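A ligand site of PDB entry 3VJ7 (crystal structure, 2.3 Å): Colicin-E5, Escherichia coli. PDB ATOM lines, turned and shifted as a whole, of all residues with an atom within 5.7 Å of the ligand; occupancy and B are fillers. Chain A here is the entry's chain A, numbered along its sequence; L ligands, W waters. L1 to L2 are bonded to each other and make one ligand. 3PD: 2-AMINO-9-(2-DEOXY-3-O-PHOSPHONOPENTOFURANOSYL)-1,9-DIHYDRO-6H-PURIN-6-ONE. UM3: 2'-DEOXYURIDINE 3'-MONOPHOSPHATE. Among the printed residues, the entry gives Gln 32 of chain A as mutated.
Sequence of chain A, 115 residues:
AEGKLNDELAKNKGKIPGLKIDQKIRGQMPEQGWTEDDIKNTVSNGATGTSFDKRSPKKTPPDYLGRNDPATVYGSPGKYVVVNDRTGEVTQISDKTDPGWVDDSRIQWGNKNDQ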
ATOM      1  N   LYS A  24     -21.480 -29.483  -5.489  1.00  0.00           N
ATOM      2  CA  LYS A  24     -20.477 -28.513  -5.072  1.00  0.00           C
ATOM      3  C   LYS A  24     -21.165 -27.154  -4.990  1.00  0.00           C
ATOM      4  O   LYS A  24     -21.072 -26.468  -3.972  1.00  0.00           O
ATOM      5  CB  LYS A  24     -19.325 -28.479  -6.075  1.00  0.00           C
ATOM      6  CG  LYS A  24     -18.019 -27.902  -5.505  1.00  0.00           C
ATOM      7  CD  LYS A  24     -17.954 -26.389  -5.595  1.00  0.00           C
ATOM      8  CE  LYS A  24     -17.738 -25.947  -7.031  1.00  0.00           C
ATOM      9  NZ  LYS A  24     -17.481 -24.488  -7.176  1.00  0.00           N
ATOM     10  N   ILE A  25     -21.874 -26.771  -6.055  1.00  0.00           N
ATOM     11  CA  ILE A  25     -22.572 -25.480  -6.081  1.00  0.00           C
ATOM     12  C   ILE A  25     -23.716 -25.427  -5.060  1.00  0.00           C
ATOM     13  O   ILE A  25     -23.930 -24.402  -4.431  1.00  0.00           O
ATOM     14  CB  ILE A  25     -23.083 -25.146  -7.520  1.00  0.00           C
ATOM     15  CG1 ILE A  25     -22.068 -24.262  -8.234  1.00  0.00           C
ATOM     16  CG2 ILE A  25     -24.401 -24.387  -7.467  1.00  0.00           C
ATOM     17  CD1 ILE A  25     -20.658 -24.780  -8.193  1.00  0.00           C
ATOM     18  N   GLN A  28     -22.404 -24.268  -1.813  1.00  0.00           N
ATOM     19  CA  GLN A  28     -21.994 -22.859  -1.725  1.00  0.00           C
ATOM     20  C   GLN A  28     -23.118 -21.826  -1.736  1.00  0.00           C
ATOM     21  O   GLN A  28     -22.905 -20.682  -1.337  1.00  0.00           O
ATOM     22  CB  GLN A  28     -21.017 -22.522  -2.864  1.00  0.00           C
ATOM     23  CG  GLN A  28     -19.716 -23.298  -2.874  1.00  0.00           C
ATOM     24  CD  GLN A  28     -18.815 -22.890  -4.029  1.00  0.00           C
ATOM     25  OE1 GLN A  28     -19.227 -22.905  -5.184  1.00  0.00           O
ATOM     26  NE2 GLN A  28     -17.578 -22.525  -3.712  1.00  0.00           N
ATOM     27  N   GLN A  32     -23.045 -18.164   0.141  1.00  0.00           N
ATOM     28  CA  GLN A  32     -22.736 -17.029  -0.733  1.00  0.00           C
ATOM     29  C   GLN A  32     -23.934 -16.151  -1.089  1.00  0.00           C
ATOM     30  O   GLN A  32     -23.857 -15.296  -1.985  1.00  0.00           O
ATOM     31  CB  GLN A  32     -22.041 -17.555  -1.995  1.00  0.00           C
ATOM     32  CG  GLN A  32     -20.731 -18.276  -1.676  1.00  0.00           C
ATOM     33  CD  GLN A  32     -20.016 -18.840  -2.899  1.00  0.00           C
ATOM     34  OE1 GLN A  32     -18.963 -19.463  -2.773  1.00  0.00           O
ATOM     35  NE2 GLN A  32     -20.590 -18.626  -4.083  1.00  0.00           N
ATOM     36  N   SER A  51     -18.394 -15.749 -21.327  1.00  0.00           N
ATOM     37  CA  SER A  51     -17.089 -16.184 -20.855  1.00  0.00           C
ATOM     38  C   SER A  51     -16.861 -17.631 -21.245  1.00  0.00           C
ATOM     39  O   SER A  51     -17.469 -18.139 -22.184  1.00  0.00           O
ATOM     40  CB  SER A  51     -16.933 -16.014 -19.348  1.00  0.00           C
ATOM     41  OG  SER A  51     -17.365 -17.156 -18.644  1.00  0.00           O
ATOM     42  N   PHE A  52     -15.990 -18.301 -20.515  1.00  0.00           N
ATOM     43  CA  PHE A  52     -15.711 -19.692 -20.801  1.00  0.00           C
ATOM     44  C   PHE A  52     -15.686 -20.493 -19.527  1.00  0.00           C
ATOM     45  O   PHE A  52     -15.339 -20.001 -18.455  1.00  0.00           O
ATOM     46  CB  PHE A  52     -14.374 -19.822 -21.542  1.00  0.00           C
ATOM     47  CG  PHE A  52     -14.276 -18.946 -22.769  1.00  0.00           C
ATOM     48  CD1 PHE A  52     -13.818 -17.637 -22.665  1.00  0.00           C
ATOM     49  CD2 PHE A  52     -14.672 -19.421 -24.015  1.00  0.00           C
ATOM     50  CE1 PHE A  52     -13.765 -16.812 -23.784  1.00  0.00           C
ATOM     51  CE2 PHE A  52     -14.626 -18.602 -25.144  1.00  0.00           C
ATOM     52  CZ  PHE A  52     -14.175 -17.290 -25.027  1.00  0.00           C
ATOM     53  N   ASP A  53     -16.115 -21.749 -19.637  1.00  0.00           N
ATOM     54  CA  ASP A  53     -16.103 -22.627 -18.494  1.00  0.00           C
ATOM     55  C   ASP A  53     -14.837 -23.452 -18.698  1.00  0.00           C
ATOM     56  O   ASP A  53     -14.770 -24.288 -19.593  1.00  0.00           O
ATOM     57  CB  ASP A  53     -17.340 -23.529 -18.500  1.00  0.00           C
ATOM     58  CG  ASP A  53     -17.359 -24.484 -17.325  1.00  0.00           C
ATOM     59  OD1 ASP A  53     -18.410 -25.127 -17.098  1.00  0.00           O
ATOM     60  OD2 ASP A  53     -16.332 -24.612 -16.650  1.00  0.00           O
ATOM     61  N   LYS A  54     -13.844 -23.170 -17.876  1.00  0.00           N
ATOM     62  CA  LYS A  54     -12.560 -23.850 -17.944  1.00  0.00           C
ATOM     63  C   LYS A  54     -12.291 -24.590 -16.638  1.00  0.00           C
ATOM     64  O   LYS A  54     -11.143 -24.727 -16.223  1.00  0.00           O
ATOM     65  CB  LYS A  54     -11.471 -22.796 -18.181  1.00  0.00           C
ATOM     66  CG  LYS A  54     -10.521 -23.111 -19.305  1.00  0.00           C
ATOM     67  CD  LYS A  54     -11.160 -22.881 -20.669  1.00  0.00           C
ATOM     68  CE  LYS A  54     -10.093 -23.083 -21.725  1.00  0.00           C
ATOM     69  NZ  LYS A  54      -8.913 -22.237 -21.419  1.00  0.00           N
ATOM     70  N   ARG A  55     -13.355 -25.065 -15.996  1.00  0.00           N
ATOM     71  CA  ARG A  55     -13.204 -25.766 -14.734  1.00  0.00           C
ATOM     72  C   ARG A  55     -12.292 -26.994 -14.785  1.00  0.00           C
ATOM     73  O   ARG A  55     -12.311 -27.763 -15.746  1.00  0.00           O
ATOM     74  CB  ARG A  55     -14.576 -26.199 -14.210  1.00  0.00           C
ATOM     75  CG  ARG A  55     -15.404 -25.081 -13.592  1.00  0.00           C
ATOM     76  CD  ARG A  55     -16.751 -25.605 -13.149  1.00  0.00           C
ATOM     77  NE  ARG A  55     -17.546 -26.009 -14.300  1.00  0.00           N
ATOM     78  CZ  ARG A  55     -18.449 -26.985 -14.287  1.00  0.00           C
ATOM     79  NH1 ARG A  55     -19.131 -27.283 -15.402  1.00  0.00           N
ATOM     80  NH2 ARG A  55     -18.671 -27.673 -13.174  1.00  0.00           N
ATOM     81  N   SER A  56     -11.510 -27.163 -13.722  1.00  0.00           N
ATOM     82  CA  SER A  56     -10.604 -28.294 -13.599  1.00  0.00           C
ATOM     83  C   SER A  56     -11.417 -29.550 -13.359  1.00  0.00           C
ATOM     84  O   SER A  56     -12.567 -29.490 -12.930  1.00  0.00           O
ATOM     85  CB  SER A  56      -9.640 -28.100 -12.428  1.00  0.00           C
ATOM     86  OG  SER A  56      -8.667 -27.123 -12.746  1.00  0.00           O
ATOM     87  N   LYS A  59     -13.363 -30.171 -10.187  1.00  0.00           N
ATOM     88  CA  LYS A  59     -14.529 -29.339  -9.957  1.00  0.00           C
ATOM     89  C   LYS A  59     -15.702 -29.608 -10.907  1.00  0.00           C
ATOM     90  O   LYS A  59     -16.637 -28.791 -10.989  1.00  0.00           O
ATOM     91  CB  LYS A  59     -14.116 -27.864 -10.014  1.00  0.00           C
ATOM     92  CG  LYS A  59     -14.962 -26.964  -9.134  1.00  0.00           C
ATOM     93  CD  LYS A  59     -14.135 -25.801  -8.613  1.00  0.00           C
ATOM     94  CE  LYS A  59     -13.005 -26.287  -7.721  1.00  0.00           C
ATOM     95  NZ  LYS A  59     -12.158 -25.169  -7.237  1.00  0.00           N
ATOM     96  N   VAL A  73     -23.078 -15.426 -19.038  1.00  0.00           N
ATOM     97  CA  VAL A  73     -23.072 -14.836 -17.710  1.00  0.00           C
ATOM     98  C   VAL A  73     -24.394 -14.134 -17.467  1.00  0.00           C
ATOM     99  O   VAL A  73     -24.928 -13.482 -18.369  1.00  0.00           O
ATOM    100  CB  VAL A  73     -21.934 -13.779 -17.566  1.00  0.00           C
ATOM    101  CG1 VAL A  73     -21.832 -13.291 -16.130  1.00  0.00           C
ATOM    102  CG2 VAL A  73     -20.618 -14.370 -18.037  1.00  0.00           C
ATOM    103  N   TYR A  80     -23.300 -12.575  -9.897  1.00  0.00           N
ATOM    104  CA  TYR A  80     -23.540 -13.261 -11.150  1.00  0.00           C
ATOM    105  C   TYR A  80     -23.593 -14.776 -11.116  1.00  0.00           C
ATOM    106  O   TYR A  80     -23.231 -15.423 -10.134  1.00  0.00           O
ATOM    107  CB  TYR A  80     -22.483 -12.827 -12.171  1.00  0.00           C
ATOM    108  CG  TYR A  80     -21.059 -13.154 -11.770  1.00  0.00           C
ATOM    109  CD1 TYR A  80     -20.251 -12.210 -11.136  1.00  0.00           C
ATOM    110  CD2 TYR A  80     -20.532 -14.418 -12.020  1.00  0.00           C
ATOM    111  CE1 TYR A  80     -18.928 -12.533 -10.748  1.00  0.00           C
ATOM    112  CE2 TYR A  80     -19.228 -14.740 -11.649  1.00  0.00           C
ATOM    113  CZ  TYR A  80     -18.438 -13.808 -11.012  1.00  0.00           C
ATOM    114  OH  TYR A  80     -17.174 -14.179 -10.609  1.00  0.00           O
ATOM    115  N   VAL A  82     -22.770 -18.094 -13.864  1.00  0.00           N
ATOM    116  CA  VAL A  82     -22.152 -18.455 -15.130  1.00  0.00           C
ATOM    117  C   VAL A  82     -22.723 -19.830 -15.505  1.00  0.00           C
ATOM    118  O   VAL A  82     -22.723 -20.750 -14.689  1.00  0.00           O
ATOM    119  CB  VAL A  82     -20.604 -18.534 -15.014  1.00  0.00           C
ATOM    120  CG1 VAL A  82     -19.997 -19.040 -16.311  1.00  0.00           C
ATOM    121  CG2 VAL A  82     -20.039 -17.153 -14.689  1.00  0.00           C
ATOM    122  N   THR A  91     -21.420 -22.981 -13.784  1.00  0.00           N
ATOM    123  CA  THR A  91     -19.988 -23.091 -13.547  1.00  0.00           C
ATOM    124  C   THR A  91     -19.568 -22.327 -12.294  1.00  0.00           C
ATOM    125  O   THR A  91     -18.694 -22.764 -11.554  1.00  0.00           O
ATOM    126  CB  THR A  91     -19.169 -22.662 -14.812  1.00  0.00           C
ATOM    127  OG1 THR A  91     -18.769 -21.283 -14.708  1.00  0.00           O
ATOM    128  CG2 THR A  91     -20.020 -22.837 -16.064  1.00  0.00           C
ATOM    129  N   GLN A  92     -20.213 -21.192 -12.031  1.00  0.00           N
ATOM    130  CA  GLN A  92     -19.886 -20.413 -10.844  1.00  0.00           C
ATOM    131  C   GLN A  92     -20.945 -19.413 -10.413  1.00  0.00           C
ATOM    132  O   GLN A  92     -21.616 -18.801 -11.232  1.00  0.00           O
ATOM    133  CB  GLN A  92     -18.556 -19.672 -11.040  1.00  0.00           C
ATOM    134  CG  GLN A  92     -18.272 -18.553 -10.017  1.00  0.00           C
ATOM    135  CD  GLN A  92     -16.906 -17.879 -10.239  1.00  0.00           C
ATOM    136  OE1 GLN A  92     -15.913 -18.275  -9.628  1.00  0.00           O
ATOM    137  NE2 GLN A  92     -16.864 -16.876 -11.101  1.00  0.00           N
ATOM    138  N   ILE A  93     -21.118 -19.289  -9.102  1.00  0.00           N
ATOM    139  CA  ILE A  93     -22.015 -18.290  -8.545  1.00  0.00           C
ATOM    140  C   ILE A  93     -21.047 -17.431  -7.730  1.00  0.00           C
ATOM    141  O   ILE A  93     -20.202 -17.966  -7.015  1.00  0.00           O
ATOM    142  CB  ILE A  93     -23.103 -18.876  -7.593  1.00  0.00           C
ATOM    143  CG1 ILE A  93     -22.451 -19.840  -6.595  1.00  0.00           C
ATOM    144  CG2 ILE A  93     -24.186 -19.584  -8.394  1.00  0.00           C
ATOM    145  CD1 ILE A  93     -23.427 -20.414  -5.597  1.00  0.00           C
ATOM    146  N   ASP A  98     -19.515 -10.991  -0.238  1.00  0.00           N
ATOM    147  CA  ASP A  98     -18.145 -10.471  -0.294  1.00  0.00           C
ATOM    148  C   ASP A  98     -18.125  -9.220  -1.167  1.00  0.00           C
ATOM    149  O   ASP A  98     -18.232  -9.298  -2.389  1.00  0.00           O
ATOM    150  CB  ASP A  98     -17.198 -11.533  -0.879  1.00  0.00           C
ATOM    151  CG  ASP A  98     -15.736 -11.110  -0.845  1.00  0.00           C
ATOM    152  OD1 ASP A  98     -15.447  -9.918  -0.626  1.00  0.00           O
ATOM    153  OD2 ASP A  98     -14.870 -11.984  -1.056  1.00  0.00           O
ATOM    154  N   GLY A 100     -15.641  -7.372  -1.754  1.00  0.00           N
ATOM    155  CA  GLY A 100     -14.381  -7.269  -2.473  1.00  0.00           C
ATOM    156  C   GLY A 100     -14.241  -8.325  -3.567  1.00  0.00           C
ATOM    157  O   GLY A 100     -13.172  -8.477  -4.154  1.00  0.00           O
ATOM    158  N   TRP A 101     -15.330  -9.028  -3.854  1.00  0.00           N
ATOM    159  CA  TRP A 101     -15.298 -10.070  -4.872  1.00  0.00           C
ATOM    160  C   TRP A 101     -14.704  -9.605  -6.195  1.00  0.00           C
ATOM    161  O   TRP A 101     -15.103  -8.566  -6.746  1.00  0.00           O
ATOM    162  CB  TRP A 101     -16.694 -10.637  -5.107  1.00  0.00           C
ATOM    163  CG  TRP A 101     -16.700 -11.800  -6.079  1.00  0.00           C
ATOM    164  CD1 TRP A 101     -16.790 -11.726  -7.441  1.00  0.00           C
ATOM    165  CD2 TRP A 101     -16.586 -13.190  -5.754  1.00  0.00           C
ATOM    166  NE1 TRP A 101     -16.754 -12.989  -7.990  1.00  0.00           N
ATOM    167  CE2 TRP A 101     -16.622 -13.908  -6.976  1.00  0.00           C
ATOM    168  CE3 TRP A 101     -16.449 -13.913  -4.557  1.00  0.00           C
ATOM    169  CZ2 TRP A 101     -16.535 -15.303  -7.038  1.00  0.00           C
ATOM    170  CZ3 TRP A 101     -16.366 -15.295  -4.616  1.00  0.00           C
ATOM    171  CH2 TRP A 101     -16.408 -15.974  -5.847  1.00  0.00           C
ATOM    172  N   VAL A 102     -13.753 -10.370  -6.712  1.00  0.00           N
ATOM    173  CA  VAL A 102     -13.146 -10.046  -7.985  1.00  0.00           C
ATOM    174  C   VAL A 102     -13.779 -10.953  -9.021  1.00  0.00           C
ATOM    175  O   VAL A 102     -13.857 -12.160  -8.824  1.00  0.00           O
ATOM    176  CB  VAL A 102     -11.636 -10.319  -7.957  1.00  0.00           C
ATOM    177  CG1 VAL A 102     -11.032 -10.009  -9.339  1.00  0.00           C
ATOM    178  CG2 VAL A 102     -10.964  -9.498  -6.856  1.00  0.00           C
ATOM    179  N   ASP A 103     -14.238 -10.369 -10.119  1.00  0.00           N
ATOM    180  CA  ASP A 103     -14.852 -11.170 -11.167  1.00  0.00           C
ATOM    181  C   ASP A 103     -13.847 -12.137 -11.778  1.00  0.00           C
ATOM    182  O   ASP A 103     -12.665 -11.841 -11.856  1.00  0.00           O
ATOM    183  CB  ASP A 103     -15.421 -10.274 -12.258  1.00  0.00           C
ATOM    184  CG  ASP A 103     -16.636  -9.497 -11.803  1.00  0.00           C
ATOM    185  OD1 ASP A 103     -17.107  -9.743 -10.666  1.00  0.00           O
ATOM    186  OD2 ASP A 103     -17.117  -8.640 -12.565  1.00  0.00           O
ATOM    187  N   ASP A 104     -14.322 -13.308 -12.207  1.00  0.00           N
ATOM    188  CA  ASP A 104     -13.436 -14.273 -12.838  1.00  0.00           C
ATOM    189  C   ASP A 104     -12.905 -13.587 -14.090  1.00  0.00           C
ATOM    190  O   ASP A 104     -13.652 -12.868 -14.768  1.00  0.00           O
ATOM    191  CB  ASP A 104     -14.203 -15.552 -13.200  1.00  0.00           C
ATOM    192  CG  ASP A 104     -13.309 -16.602 -13.842  1.00  0.00           C
ATOM    193  OD1 ASP A 104     -13.235 -16.648 -15.086  1.00  0.00           O
ATOM    194  OD2 ASP A 104     -12.683 -17.371 -13.089  1.00  0.00           O
ATOM    195  N   ARG A 106     -12.287 -14.613 -17.012  1.00  0.00           N
ATOM    196  CA  ARG A 106     -12.810 -15.020 -18.302  1.00  0.00           C
ATOM    197  C   ARG A 106     -14.087 -14.282 -18.658  1.00  0.00           C
ATOM    198  O   ARG A 106     -14.484 -14.247 -19.817  1.00  0.00           O
ATOM    199  CB  ARG A 106     -13.021 -16.530 -18.330  1.00  0.00           C
ATOM    200  CG  ARG A 106     -11.749 -17.291 -17.956  1.00  0.00           C
ATOM    201  CD  ARG A 106     -11.958 -18.782 -17.917  1.00  0.00           C
ATOM    202  NE  ARG A 106     -10.890 -19.455 -17.179  1.00  0.00           N
ATOM    203  CZ  ARG A 106     -10.790 -19.461 -15.857  1.00  0.00           C
ATOM    204  NH1 ARG A 106     -11.700 -18.853 -15.112  1.00  0.00           N
ATOM    205  NH2 ARG A 106      -9.787 -20.095 -15.273  1.00  0.00           N
ATOM    206  N   ILE A 107     -14.723 -13.681 -17.650  1.00  0.00           N
ATOM    207  CA  ILE A 107     -15.977 -12.953 -17.877  1.00  0.00           C
ATOM    208  C   ILE A 107     -15.813 -11.686 -18.722  1.00  0.00           C
ATOM    209  O   ILE A 107     -14.945 -10.859 -18.462  1.00  0.00           O
ATOM    210  CB  ILE A 107     -16.626 -12.542 -16.548  1.00  0.00           C
ATOM    211  CG1 ILE A 107     -17.076 -13.783 -15.777  1.00  0.00           C
ATOM    212  CG2 ILE A 107     -17.820 -11.637 -16.814  1.00  0.00           C
ATOM    213  CD1 ILE A 107     -17.566 -13.471 -14.398  1.00  0.00           C
HETATM  214  O5' 3PD L   1     -11.459 -18.513  -8.579  1.00  0.00           O
HETATM  215  C5' 3PD L   1     -11.081 -19.743  -7.960  1.00  0.00           C
HETATM  216  C4' 3PD L   1     -11.919 -20.019  -6.718  1.00  0.00           C
HETATM  217  O4' 3PD L   1     -11.558 -19.151  -5.605  1.00  0.00           O
HETATM  218  C1' 3PD L   1     -12.678 -18.766  -4.874  1.00  0.00           C
HETATM  219  C2' 3PD L   1     -13.940 -19.365  -5.515  1.00  0.00           C
HETATM  220  C3' 3PD L   1     -13.449 -19.865  -6.896  1.00  0.00           C
HETATM  221  O3' 3PD L   1     -13.941 -21.172  -7.235  1.00  0.00           O
HETATM  222  N9  3PD L   1     -12.675 -17.244  -4.712  1.00  0.00           N
HETATM  223  C4  3PD L   1     -12.849 -16.244  -5.674  1.00  0.00           C
HETATM  224  N3  3PD L   1     -13.108 -16.431  -7.050  1.00  0.00           N
HETATM  225  C2  3PD L   1     -13.246 -15.249  -7.736  1.00  0.00           C
HETATM  226  N2  3PD L   1     -13.490 -15.225  -9.045  1.00  0.00           N
HETATM  227  N1  3PD L   1     -13.162 -14.005  -7.107  1.00  0.00           N
HETATM  228  C6  3PD L   1     -12.910 -13.781  -5.710  1.00  0.00           C
HETATM  229  O6  3PD L   1     -12.860 -12.621  -5.283  1.00  0.00           O
HETATM  230  C5  3PD L   1     -12.758 -15.022  -4.968  1.00  0.00           C
HETATM  231  N7  3PD L   1     -12.502 -15.242  -3.622  1.00  0.00           N
HETATM  232  C8  3PD L   1     -12.475 -16.553  -3.531  1.00  0.00           C
HETATM  233  P   3PD L   1     -15.477 -21.647  -7.228  1.00  0.00           P
HETATM  234  O1P 3PD L   1     -15.631 -22.620  -6.147  1.00  0.00           O
HETATM  235  O1  3PD L   1     -16.432 -20.507  -7.218  1.00  0.00           O
HETATM  236  N1  UM3 L   2     -14.821 -20.613 -13.721  1.00  0.00           N
HETATM  237  C2  UM3 L   2     -14.744 -20.695 -15.144  1.00  0.00           C
HETATM  238  N3  UM3 L   2     -15.385 -19.642 -15.827  1.00  0.00           N
HETATM  239  C4  UM3 L   2     -16.070 -18.561 -15.257  1.00  0.00           C
HETATM  240  C5  UM3 L   2     -16.103 -18.543 -13.786  1.00  0.00           C
HETATM  241  C6  UM3 L   2     -15.501 -19.541 -13.069  1.00  0.00           C
HETATM  242  O2  UM3 L   2     -14.177 -21.597 -15.746  1.00  0.00           O
HETATM  243  O4  UM3 L   2     -16.594 -17.728 -15.970  1.00  0.00           O
HETATM  244  C1' UM3 L   2     -14.153 -21.748 -12.948  1.00  0.00           C
HETATM  245  C2' UM3 L   2     -13.016 -21.411 -11.972  1.00  0.00           C
HETATM  246  C3' UM3 L   2     -13.262 -22.459 -10.861  1.00  0.00           C
HETATM  247  C4' UM3 L   2     -14.800 -22.547 -10.838  1.00  0.00           C
HETATM  248  O3' UM3 L   2     -12.796 -23.782 -11.236  1.00  0.00           O
HETATM  249  O4' UM3 L   2     -15.191 -22.384 -12.223  1.00  0.00           O
HETATM  250  C5' UM3 L   2     -15.479 -21.638  -9.863  1.00  0.00           C
HETATM  251  O5' UM3 L   2     -15.588 -22.390  -8.626  1.00  0.00           O
HETATM  252  P   UM3 L   2     -11.266 -23.982 -11.260  1.00  0.00           P
HETATM  253  O1P UM3 L   2     -11.024 -25.345 -11.646  1.00  0.00           O
HETATM  254  O2P UM3 L   2     -10.759 -23.756  -9.933  1.00  0.00           O
HETATM  255  O3P UM3 L   2     -10.601 -23.106 -12.187  1.00  0.00           O
HETATM  256  O   HOH W   1     -13.961 -22.947  -3.899  1.00  0.00           O
HETATM  257  O   HOH W   2      -8.742 -24.836  -8.703  1.00  0.00           O
HETATM  258  O   HOH W   3     -19.127 -21.237  -7.609  1.00  0.00           O
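An oxygen (O6) of 3PD L1 is in hydrogen-bond range of the backbone NH (N) of Val 102 (2.8 Å). The backbone carbonyl oxygen (O) of Val 102 lies within hydrogen-bond range of a nitrogen (N1) of 3PD L1, 2.6 Å away. O of Phe 52 sits at hydrogen-bond distance from N3 of UM3 L2. The backbone NH of Lys 54 sits at hydrogen-bond distance from an oxygen (O2) of UM3 L2 (2.7 Å). The backbone NH (N) of Ser 56 lies within hydrogen-bond range of an oxygen (O1P) of UM3 L2, 2.8 Å away. The side-chain hydroxyl of Ser 56 sits at hydrogen-bond distance from an oxygen (O1P) of UM3 L2 (3.2 Å). O1P of 3PD L1 is in salt-bridge range of NZ of Lys 24. An oxygen (O4) of UM3 L2 lies within hydrogen-bond range of the side-chain hydroxyl (OG) of Ser 51 (2.8 Å). The side-chain amide nitrogen (NE2) of Gln 28 is in hydrogen-bond range of an oxygen (O1P) of 3PD L1 (3.1 Å). O1 of 3PD L1 sits close to OE1 of Gln 92 (3.3 Å). NZ of Lys 59 is in salt-bridge range of O2P of UM3 L2 (3.3 Å).
NH1 of Arg 55 is in salt-bridge range of OD1 of Asp 53, at 2.8 Å. The backbone carbonyl oxygen (O) of Gln 92 lies within hydrogen-bond range of the backbone NH (N) of Val 82 (3.0 Å). The side-chain amide nitrogen (NE2) of Gln 92 sits at hydrogen-bond distance from the side-chain hydroxyl (OH) of Tyr 80. NE1 of Trp 101 sits at hydrogen-bond distance from OH of Tyr 80, 2.9 Å away. The side-chain carboxylate of Asp 98 is in hydrogen-bond range of the backbone NH of Trp 101, at 3.4 Å. The guanidinium group of Arg 106 lies within salt-bridge range of the side-chain carboxylate of Asp 104, 2.7 Å away. N of Asp 104 sits at hydrogen-bond distance from OH of Tyr 80 (3.4 Å). N of Thr 91 lies within hydrogen-bond range of O of Val 82, at 2.7 Å.
Asp 53 touches the ligand. CG of Arg 55 touches O4' of UM3 L2, at 3.0 Å. Val 82 touches the ligand. O of Thr 91 touches O4' of UM3 L2 (3.6 Å). Trp 101 touches the ligand. CG of Asp 104 touches C5 of UM3 L2, at 3.4 Å. NH1 of Arg 106 touches C2 of UM3 L2, at 3.6 Å. CG1 of Ile 107 touches O4 of UM3 L2 (3.98 Å). Hydrophobic or aromatic side chains within 4 Å of the ligand: Val 82, Trp 101, Val 102 and Ile 107.
Water W3 lies within hydrogen-bond range of an oxygen (O1) of 3PD L1 (2.8 Å), the side-chain amide oxygen of Gln 28 (2.9 Å) and the backbone NH of Ile 93 (3.2 Å).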
